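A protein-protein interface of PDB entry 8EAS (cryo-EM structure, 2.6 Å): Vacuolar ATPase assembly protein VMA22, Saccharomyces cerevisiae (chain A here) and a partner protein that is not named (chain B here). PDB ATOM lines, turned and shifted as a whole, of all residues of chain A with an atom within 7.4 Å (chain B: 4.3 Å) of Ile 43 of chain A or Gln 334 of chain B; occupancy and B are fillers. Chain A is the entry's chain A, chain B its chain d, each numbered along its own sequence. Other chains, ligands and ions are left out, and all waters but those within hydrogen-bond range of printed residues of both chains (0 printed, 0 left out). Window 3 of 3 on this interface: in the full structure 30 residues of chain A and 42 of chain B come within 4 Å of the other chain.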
ATOM      1  N   GLN A  35       8.487  25.635 -26.383  1.00  0.00           N
ATOM      2  CA  GLN A  35       8.852  24.537 -25.502  1.00  0.00           C
ATOM      3  C   GLN A  35       9.121  25.042 -24.096  1.00  0.00           C
ATOM      4  O   GLN A  35       8.677  24.431 -23.124  1.00  0.00           O
ATOM      5  CB  GLN A  35      10.067  23.797 -26.055  1.00  0.00           C
ATOM      6  CG  GLN A  35      10.538  22.643 -25.194  1.00  0.00           C
ATOM      7  CD  GLN A  35       9.556  21.486 -25.181  1.00  0.00           C
ATOM      8  OE1 GLN A  35       9.618  20.599 -26.029  1.00  0.00           O
ATOM      9  NE2 GLN A  35       8.651  21.485 -24.213  1.00  0.00           N
ATOM     10  N   LYS A  36       9.830  26.165 -23.962  1.00  0.00           N
ATOM     11  CA  LYS A  36      10.062  26.727 -22.635  1.00  0.00           C
ATOM     12  C   LYS A  36       8.755  27.122 -21.963  1.00  0.00           C
ATOM     13  O   LYS A  36       8.566  26.877 -20.765  1.00  0.00           O
ATOM     14  CB  LYS A  36      11.000  27.927 -22.721  1.00  0.00           C
ATOM     15  CG  LYS A  36      11.303  28.551 -21.372  1.00  0.00           C
ATOM     16  CD  LYS A  36      12.156  27.632 -20.520  1.00  0.00           C
ATOM     17  CE  LYS A  36      12.550  28.295 -19.214  1.00  0.00           C
ATOM     18  NZ  LYS A  36      13.333  27.375 -18.341  1.00  0.00           N
ATOM     19  N   GLY A  37       7.839  27.731 -22.717  1.00  0.00           N
ATOM     20  CA  GLY A  37       6.558  28.106 -22.146  1.00  0.00           C
ATOM     21  C   GLY A  37       5.746  26.909 -21.697  1.00  0.00           C
ATOM     22  O   GLY A  37       5.165  26.915 -20.611  1.00  0.00           O
ATOM     23  N   PHE A  38       5.696  25.864 -22.524  1.00  0.00           N
ATOM     24  CA  PHE A  38       4.971  24.661 -22.138  1.00  0.00           C
ATOM     25  C   PHE A  38       5.621  23.972 -20.948  1.00  0.00           C
ATOM     26  O   PHE A  38       4.919  23.463 -20.074  1.00  0.00           O
ATOM     27  CB  PHE A  38       4.848  23.698 -23.316  1.00  0.00           C
ATOM     28  CG  PHE A  38       3.630  23.929 -24.162  1.00  0.00           C
ATOM     29  CD1 PHE A  38       2.405  23.429 -23.774  1.00  0.00           C
ATOM     30  CD2 PHE A  38       3.710  24.626 -25.349  1.00  0.00           C
ATOM     31  CE1 PHE A  38       1.284  23.630 -24.545  1.00  0.00           C
ATOM     32  CE2 PHE A  38       2.590  24.827 -26.125  1.00  0.00           C
ATOM     33  CZ  PHE A  38       1.378  24.330 -25.720  1.00  0.00           C
ATOM     34  N   GLN A  39       6.953  23.933 -20.895  1.00  0.00           N
ATOM     35  CA  GLN A  39       7.628  23.354 -19.737  1.00  0.00           C
ATOM     36  C   GLN A  39       7.282  24.114 -18.468  1.00  0.00           C
ATOM     37  O   GLN A  39       6.982  23.509 -17.434  1.00  0.00           O
ATOM     38  CB  GLN A  39       9.139  23.348 -19.955  1.00  0.00           C
ATOM     39  CG  GLN A  39       9.603  22.508 -21.113  1.00  0.00           C
ATOM     40  CD  GLN A  39      11.093  22.290 -21.097  1.00  0.00           C
ATOM     41  OE1 GLN A  39      11.816  22.935 -20.339  1.00  0.00           O
ATOM     42  NE2 GLN A  39      11.567  21.385 -21.942  1.00  0.00           N
ATOM     43  N   ASP A  40       7.320  25.446 -18.528  1.00  0.00           N
ATOM     44  CA  ASP A  40       6.969  26.245 -17.361  1.00  0.00           C
ATOM     45  C   ASP A  40       5.528  25.996 -16.949  1.00  0.00           C
ATOM     46  O   ASP A  40       5.232  25.799 -15.767  1.00  0.00           O
ATOM     47  CB  ASP A  40       7.188  27.726 -17.655  1.00  0.00           C
ATOM     48  CG  ASP A  40       8.628  28.052 -17.955  1.00  0.00           C
ATOM     49  OD1 ASP A  40       9.506  27.229 -17.623  1.00  0.00           O
ATOM     50  OD2 ASP A  40       8.882  29.132 -18.526  1.00  0.00           O
ATOM     51  N   GLY A  41       4.616  25.984 -17.920  1.00  0.00           N
ATOM     52  CA  GLY A  41       3.218  25.764 -17.605  1.00  0.00           C
ATOM     53  C   GLY A  41       2.959  24.394 -17.018  1.00  0.00           C
ATOM     54  O   GLY A  41       2.205  24.257 -16.057  1.00  0.00           O
ATOM     55  N   TYR A  42       3.578  23.361 -17.587  1.00  0.00           N
ATOM     56  CA  TYR A  42       3.391  22.008 -17.083  1.00  0.00           C
ATOM     57  C   TYR A  42       3.976  21.845 -15.692  1.00  0.00           C
ATOM     58  O   TYR A  42       3.365  21.205 -14.833  1.00  0.00           O
ATOM     59  CB  TYR A  42       4.012  20.993 -18.038  1.00  0.00           C
ATOM     60  CG  TYR A  42       3.257  20.833 -19.325  1.00  0.00           C
ATOM     61  CD1 TYR A  42       1.875  20.788 -19.336  1.00  0.00           C
ATOM     62  CD2 TYR A  42       3.926  20.728 -20.527  1.00  0.00           C
ATOM     63  CE1 TYR A  42       1.186  20.649 -20.511  1.00  0.00           C
ATOM     64  CE2 TYR A  42       3.248  20.590 -21.702  1.00  0.00           C
ATOM     65  CZ  TYR A  42       1.882  20.550 -21.693  1.00  0.00           C
ATOM     66  OH  TYR A  42       1.215  20.407 -22.881  1.00  0.00           O
ATOM     67  N   ILE A  43       5.165  22.395 -15.447  1.00  0.00           N
ATOM     68  CA  ILE A  43       5.757  22.208 -14.132  1.00  0.00           C
ATOM     69  C   ILE A  43       5.007  23.021 -13.091  1.00  0.00           C
ATOM     70  O   ILE A  43       4.884  22.597 -11.941  1.00  0.00           O
ATOM     71  CB  ILE A  43       7.264  22.524 -14.151  1.00  0.00           C
ATOM     72  CG1 ILE A  43       7.940  21.836 -12.972  1.00  0.00           C
ATOM     73  CG2 ILE A  43       7.522  24.018 -14.111  1.00  0.00           C
ATOM     74  CD1 ILE A  43       7.700  20.345 -12.925  1.00  0.00           C
ATOM     75  N   GLN A  44       4.449  24.170 -13.474  1.00  0.00           N
ATOM     76  CA  GLN A  44       3.662  24.948 -12.528  1.00  0.00           C
ATOM     77  C   GLN A  44       2.284  24.336 -12.307  1.00  0.00           C
ATOM     78  O   GLN A  44       1.727  24.449 -11.215  1.00  0.00           O
ATOM     79  CB  GLN A  44       3.574  26.384 -13.026  1.00  0.00           C
ATOM     80  CG  GLN A  44       4.895  27.107 -12.901  1.00  0.00           C
ATOM     81  CD  GLN A  44       4.995  28.310 -13.806  1.00  0.00           C
ATOM     82  OE1 GLN A  44       4.152  28.519 -14.673  1.00  0.00           O
ATOM     83  NE2 GLN A  44       6.042  29.101 -13.623  1.00  0.00           N
ATOM     84  N   LEU A  45       1.735  23.652 -13.309  1.00  0.00           N
ATOM     85  CA  LEU A  45       0.511  22.888 -13.107  1.00  0.00           C
ATOM     86  C   LEU A  45       0.755  21.690 -12.198  1.00  0.00           C
ATOM     87  O   LEU A  45      -0.072  21.373 -11.334  1.00  0.00           O
ATOM     88  CB  LEU A  45      -0.041  22.449 -14.459  1.00  0.00           C
ATOM     89  CG  LEU A  45      -1.368  21.708 -14.510  1.00  0.00           C
ATOM     90  CD1 LEU A  45      -2.448  22.538 -13.870  1.00  0.00           C
ATOM     91  CD2 LEU A  45      -1.705  21.392 -15.948  1.00  0.00           C
ATOM     92  N   SER A  46       1.896  21.024 -12.369  1.00  0.00           N
ATOM     93  CA  SER A  46       2.284  19.954 -11.461  1.00  0.00           C
ATOM     94  C   SER A  46       2.471  20.477 -10.046  1.00  0.00           C
ATOM     95  O   SER A  46       2.028  19.851  -9.081  1.00  0.00           O
ATOM     96  CB  SER A  46       3.565  19.294 -11.956  1.00  0.00           C
ATOM     97  OG  SER A  46       3.348  18.615 -13.173  1.00  0.00           O
ATOM     98  N   ARG A  47       3.128  21.626  -9.906  1.00  0.00           N
ATOM     99  CA  ARG A  47       3.300  22.255  -8.605  1.00  0.00           C
ATOM    100  C   ARG A  47       1.995  22.814  -8.064  1.00  0.00           C
ATOM    101  O   ARG A  47       1.942  23.201  -6.897  1.00  0.00           O
ATOM    102  CB  ARG A  47       4.351  23.356  -8.697  1.00  0.00           C
ATOM    103  CG  ARG A  47       4.903  23.800  -7.364  1.00  0.00           C
ATOM    104  CD  ARG A  47       5.559  22.664  -6.620  1.00  0.00           C
ATOM    105  NE  ARG A  47       6.177  23.134  -5.390  1.00  0.00           N
ATOM    106  CZ  ARG A  47       6.872  22.377  -4.556  1.00  0.00           C
ATOM    107  NH1 ARG A  47       7.081  21.096  -4.796  1.00  0.00           N
ATOM    108  NH2 ARG A  47       7.369  22.920  -3.452  1.00  0.00           N
ATOM    109  N   SER A  48       0.969  22.924  -8.905  1.00  0.00           N
ATOM    110  CA  SER A  48      -0.382  23.189  -8.432  1.00  0.00           C
ATOM    111  C   SER A  48      -1.056  21.920  -7.939  1.00  0.00           C
ATOM    112  O   SER A  48      -1.918  21.985  -7.059  1.00  0.00           O
ATOM    113  CB  SER A  48      -1.214  23.812  -9.545  1.00  0.00           C
ATOM    114  OG  SER A  48      -0.635  25.018  -9.973  1.00  0.00           O
ATOM    115  N   ASN A  49      -0.687  20.767  -8.500  1.00  0.00           N
ATOM    116  CA  ASN A  49      -1.138  19.498  -7.936  1.00  0.00           C
ATOM    117  C   ASN A  49      -0.505  19.244  -6.572  1.00  0.00           C
ATOM    118  O   ASN A  49      -1.162  18.734  -5.661  1.00  0.00           O
ATOM    119  CB  ASN A  49      -0.838  18.365  -8.910  1.00  0.00           C
ATOM    120  CG  ASN A  49      -1.469  18.592 -10.256  1.00  0.00           C
ATOM    121  OD1 ASN A  49      -2.498  19.246 -10.358  1.00  0.00           O
ATOM    122  ND2 ASN A  49      -0.853  18.059 -11.299  1.00  0.00           N
ATOM    123  N   SER A 145       0.765  29.057  -7.990  1.00  0.00           N
ATOM    124  CA  SER A 145       1.436  28.319  -9.052  1.00  0.00           C
ATOM    125  C   SER A 145       0.488  28.021 -10.205  1.00  0.00           C
ATOM    126  O   SER A 145       0.918  27.935 -11.357  1.00  0.00           O
ATOM    127  CB  SER A 145       2.039  27.034  -8.491  1.00  0.00           C
ATOM    128  OG  SER A 145       1.033  26.190  -7.971  1.00  0.00           O
ATOM    129  N   SER A 149       1.112  29.023 -14.003  1.00  0.00           N
ATOM    130  CA  SER A 149       0.935  28.083 -15.102  1.00  0.00           C
ATOM    131  C   SER A 149       0.034  28.666 -16.180  1.00  0.00           C
ATOM    132  O   SER A 149       0.314  28.536 -17.379  1.00  0.00           O
ATOM    133  CB  SER A 149       0.362  26.776 -14.562  1.00  0.00           C
ATOM    134  OG  SER A 149       0.143  25.844 -15.596  1.00  0.00           O
ATOM    135  N   SER A 152       2.005  31.083 -18.165  1.00  0.00           N
ATOM    136  CA  SER A 152       2.906  30.417 -19.099  1.00  0.00           C
ATOM    137  C   SER A 152       2.161  29.924 -20.334  1.00  0.00           C
ATOM    138  O   SER A 152       2.647  30.064 -21.462  1.00  0.00           O
ATOM    139  CB  SER A 152       3.614  29.265 -18.396  1.00  0.00           C
ATOM    140  OG  SER A 152       4.233  29.714 -17.206  1.00  0.00           O
ATOM    141  N   PHE A 153       0.967  29.362 -20.149  1.00  0.00           N
ATOM    142  CA  PHE A 153       0.220  28.861 -21.302  1.00  0.00           C
ATOM    143  C   PHE A 153      -0.352  30.003 -22.142  1.00  0.00           C
ATOM    144  O   PHE A 153      -0.389  29.924 -23.382  1.00  0.00           O
ATOM    145  CB  PHE A 153      -0.877  27.916 -20.825  1.00  0.00           C
ATOM    146  CG  PHE A 153      -0.356  26.596 -20.342  1.00  0.00           C
ATOM    147  CD1 PHE A 153       0.280  25.731 -21.211  1.00  0.00           C
ATOM    148  CD2 PHE A 153      -0.493  26.223 -19.021  1.00  0.00           C
ATOM    149  CE1 PHE A 153       0.762  24.522 -20.770  1.00  0.00           C
ATOM    150  CE2 PHE A 153      -0.009  25.015 -18.579  1.00  0.00           C
ATOM    151  CZ  PHE A 153       0.616  24.165 -19.454  1.00  0.00           C
ATOM    152  N   TRP B 325       5.135  14.929  -6.535  1.00  0.00           N
ATOM    153  CA  TRP B 325       6.029  15.977  -7.011  1.00  0.00           C
ATOM    154  C   TRP B 325       7.330  15.396  -7.541  1.00  0.00           C
ATOM    155  O   TRP B 325       7.857  15.851  -8.558  1.00  0.00           O
ATOM    156  CB  TRP B 325       6.326  16.978  -5.899  1.00  0.00           C
ATOM    157  CG  TRP B 325       7.250  18.045  -6.364  1.00  0.00           C
ATOM    158  CD1 TRP B 325       8.474  18.346  -5.855  1.00  0.00           C
ATOM    159  CD2 TRP B 325       7.031  18.953  -7.446  1.00  0.00           C
ATOM    160  NE1 TRP B 325       9.035  19.381  -6.554  1.00  0.00           N
ATOM    161  CE2 TRP B 325       8.165  19.775  -7.535  1.00  0.00           C
ATOM    162  CE3 TRP B 325       5.986  19.150  -8.349  1.00  0.00           C
ATOM    163  CZ2 TRP B 325       8.280  20.777  -8.485  1.00  0.00           C
ATOM    164  CZ3 TRP B 325       6.105  20.136  -9.286  1.00  0.00           C
ATOM    165  CH2 TRP B 325       7.243  20.940  -9.352  1.00  0.00           C
ATOM    166  N   CYS B 329       8.872  15.739 -11.250  1.00  0.00           N
ATOM    167  CA  CYS B 329      10.243  16.157 -11.505  1.00  0.00           C
ATOM    168  C   CYS B 329      11.111  15.027 -12.027  1.00  0.00           C
ATOM    169  O   CYS B 329      12.315  15.213 -12.211  1.00  0.00           O
ATOM    170  CB  CYS B 329      10.861  16.734 -10.234  1.00  0.00           C
ATOM    171  SG  CYS B 329      10.106  18.236  -9.684  1.00  0.00           S
ATOM    172  N   GLN B 332       8.866  15.156 -16.105  1.00  0.00           N
ATOM    173  CA  GLN B 332       9.052  16.406 -16.824  1.00  0.00           C
ATOM    174  C   GLN B 332      10.498  16.869 -16.853  1.00  0.00           C
ATOM    175  O   GLN B 332      10.746  18.038 -17.155  1.00  0.00           O
ATOM    176  CB  GLN B 332       8.189  17.503 -16.201  1.00  0.00           C
ATOM    177  CG  GLN B 332       6.724  17.378 -16.512  1.00  0.00           C
ATOM    178  CD  GLN B 332       5.857  18.117 -15.535  1.00  0.00           C
ATOM    179  OE1 GLN B 332       5.231  19.105 -15.878  1.00  0.00           O
ATOM    180  NE2 GLN B 332       5.806  17.637 -14.310  1.00  0.00           N
ATOM    181  N   ASN B 333      11.450  15.981 -16.575  1.00  0.00           N
ATOM    182  CA  ASN B 333      12.800  16.384 -16.210  1.00  0.00           C
ATOM    183  C   ASN B 333      12.649  17.311 -15.015  1.00  0.00           C
ATOM    184  O   ASN B 333      12.036  16.915 -14.027  1.00  0.00           O
ATOM    185  CB  ASN B 333      13.540  17.033 -17.375  1.00  0.00           C
ATOM    186  CG  ASN B 333      15.026  16.733 -17.358  1.00  0.00           C
ATOM    187  OD1 ASN B 333      15.678  16.814 -16.319  1.00  0.00           O
ATOM    188  ND2 ASN B 333      15.567  16.374 -18.515  1.00  0.00           N
ATOM    189  N   GLN B 334      13.140  18.543 -15.088  1.00  0.00           N
ATOM    190  CA  GLN B 334      12.954  19.509 -14.002  1.00  0.00           C
ATOM    191  C   GLN B 334      13.518  18.978 -12.685  1.00  0.00           C
ATOM    192  O   GLN B 334      12.847  18.971 -11.655  1.00  0.00           O
ATOM    193  CB  GLN B 334      11.478  19.882 -13.831  1.00  0.00           C
ATOM    194  CG  GLN B 334      10.775  20.340 -15.082  1.00  0.00           C
ATOM    195  CD  GLN B 334      11.107  21.758 -15.444  1.00  0.00           C
ATOM    196  OE1 GLN B 334      11.481  22.555 -14.587  1.00  0.00           O
ATOM    197  NE2 GLN B 334      10.960  22.092 -16.717  1.00  0.00           N
ATOM    198  N   ARG B 335      14.766  18.527 -12.724  1.00  0.00           N
ATOM    199  CA  ARG B 335      15.388  17.959 -11.538  1.00  0.00           C
ATOM    200  C   ARG B 335      15.955  19.010 -10.597  1.00  0.00           C
ATOM    201  O   ARG B 335      16.537  18.644  -9.572  1.00  0.00           O
ATOM    202  CB  ARG B 335      16.488  16.981 -11.942  1.00  0.00           C
ATOM    203  CG  ARG B 335      15.969  15.698 -12.553  1.00  0.00           C
ATOM    204  CD  ARG B 335      17.069  14.661 -12.636  1.00  0.00           C
ATOM    205  NE  ARG B 335      17.566  14.291 -11.318  1.00  0.00           N
ATOM    206  CZ  ARG B 335      16.979  13.411 -10.523  1.00  0.00           C
ATOM    207  NH1 ARG B 335      15.880  12.773 -10.889  1.00  0.00           N
ATOM    208  NH2 ARG B 335      17.511  13.161  -9.330  1.00  0.00           N
ATOM    209  N   GLU B 336      15.843  20.296 -10.928  1.00  0.00           N
ATOM    210  CA  GLU B 336      16.252  21.327  -9.983  1.00  0.00           C
ATOM    211  C   GLU B 336      15.208  21.543  -8.897  1.00  0.00           C
ATOM    212  O   GLU B 336      15.556  21.936  -7.778  1.00  0.00           O
ATOM    213  CB  GLU B 336      16.535  22.646 -10.710  1.00  0.00           C
ATOM    214  CG  GLU B 336      15.373  23.222 -11.514  1.00  0.00           C
ATOM    215  CD  GLU B 336      15.137  22.515 -12.836  1.00  0.00           C
ATOM    216  OE1 GLU B 336      14.190  22.902 -13.552  1.00  0.00           O
ATOM    217  OE2 GLU B 336      15.898  21.581 -13.164  1.00  0.00           O
ATOM    218  N   ARG B 337      13.942  21.287  -9.199  1.00  0.00           N
ATOM    219  CA  ARG B 337      12.853  21.455  -8.251  1.00  0.00           C
ATOM    220  C   ARG B 337      12.478  20.160  -7.553  1.00  0.00           C
ATOM    221  O   ARG B 337      11.492  20.133  -6.814  1.00  0.00           O
ATOM    222  CB  ARG B 337      11.627  22.022  -8.966  1.00  0.00           C
ATOM    223  CG  ARG B 337      11.955  23.115  -9.956  1.00  0.00           C
ATOM    224  CD  ARG B 337      10.984  23.103 -11.107  1.00  0.00           C
ATOM    225  NE  ARG B 337       9.662  23.554 -10.698  1.00  0.00           N
ATOM    226  CZ  ARG B 337       9.247  24.811 -10.761  1.00  0.00           C
ATOM    227  NH1 ARG B 337      10.030  25.771 -11.221  1.00  0.00           N
ATOM    228  NH2 ARG B 337       8.018  25.109 -10.352  1.00  0.00           N
ATOM    229  N   ILE B 338      13.246  19.094  -7.769  1.00  0.00           N
ATOM    230  CA  ILE B 338      12.867  17.775  -7.281  1.00  0.00           C
ATOM    231  C   ILE B 338      12.929  17.705  -5.761  1.00  0.00           C
ATOM    232  O   ILE B 338      12.259  16.869  -5.146  1.00  0.00           O
ATOM    233  CB  ILE B 338      13.760  16.715  -7.946  1.00  0.00           C
ATOM    234  CG1 ILE B 338      13.183  15.317  -7.746  1.00  0.00           C
ATOM    235  CG2 ILE B 338      15.174  16.817  -7.434  1.00  0.00           C
ATOM    236  CD1 ILE B 338      13.505  14.376  -8.860  1.00  0.00           C
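OG of Ser 46 of chain A lies within hydrogen-bond range of NE2 of Gln 332 of chain B, at 2.9 Å. NH1 of Arg 47 of chain A lies close to NE1 of Trp 325 of chain B. The backbone carbonyl oxygen of Tyr 42 of chain A lies close to the side-chain amide oxygen of Gln 332 of chain B, at 3.0 Å. The backbone NH of Ile 43 of chain A sits at hydrogen-bond distance from the side-chain amide oxygen of Gln 332 of chain B (3.3 Å).
The indole nitrogen of Trp 325 of chain B is in hydrogen-bond range of the backbone carbonyl oxygen of Arg 337 of chain B (2.6 Å). The backbone carbonyl oxygen (O) of Tyr 42 of chain A sits at hydrogen-bond distance from the side-chain hydroxyl (OG) of Ser 46 of chain A. The side-chain sulfur of Cys 329 of chain B is in hydrogen-bond range of the backbone carbonyl oxygen of Arg 337 of chain B (3.7 Å). The side-chain sulfur (SG) of Cys 329 of chain B lies close to the backbone carbonyl oxygen (O) of Gln 334 of chain B, at 3.5 Å. The side-chain carboxylate (OE1) of Glu 336 of chain B sits close to the side-chain amide oxygen (OE1) of Gln 334 of chain B. O of Trp 325 of chain B lies close to SG of Cys 329 of chain B, 3.5 Å away.
Gln 39 of chain A touches Gln 334 of chain B. Trp 325 of chain B touches Ile 43 of chain A. Gln 334 of chain B touches Ile 43 of chain A. Arg 337 of chain B touches Ile 43 of chain A. Trp 325 of chain B touches Ser 46 of chain A (CZ3 to C, 3.7 Å).
Ile 43 of chain A touches just these residues of chain B: Trp 325, Gln 332, Gln 334 and Arg 337. Of the printed residues of chain A, Gln 334 of chain B touches Gln 39 (3.8 Å) and Ile 43 (3.8 Å). Of the printed residues of chain B, Ser 46 of chain A touches Trp 325 and Gln 332. Of the printed residues of chain B, Arg 47 of chain A touches Trp 325. Leu 45 of chain A touches none of the printed residues of chain B. The nearest printed residue of chain B that does not touch Ile 43 of chain A is Cys 329 of chain B (4.6 Å). The nearest residue of chain A that does not touch Gln 334 of chain B is Asp 40 of chain A (5.3 Å).
Printed residues of chain B that touch a printed residue of chain A: Trp 325, Gln 332, Gln 334 and Arg 337. Of the 19 printed residues of chain A, 5 touch a printed residue of chain B. Printed residues of chain A that touch a printed residue of chain B: Gln 39, Tyr 42, Ile 43, Ser 46 and Arg 47. Hydrophobic or aromatic side chains of chain A that line the printed part of chain B: Tyr 42 and Ile 43. Among the printed residues, 9 pairs touch across the chains. Among the printed residues, no Asp or Glu carboxylate lies within 4 Å of a Lys or Arg side-chain nitrogen of the other chain.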
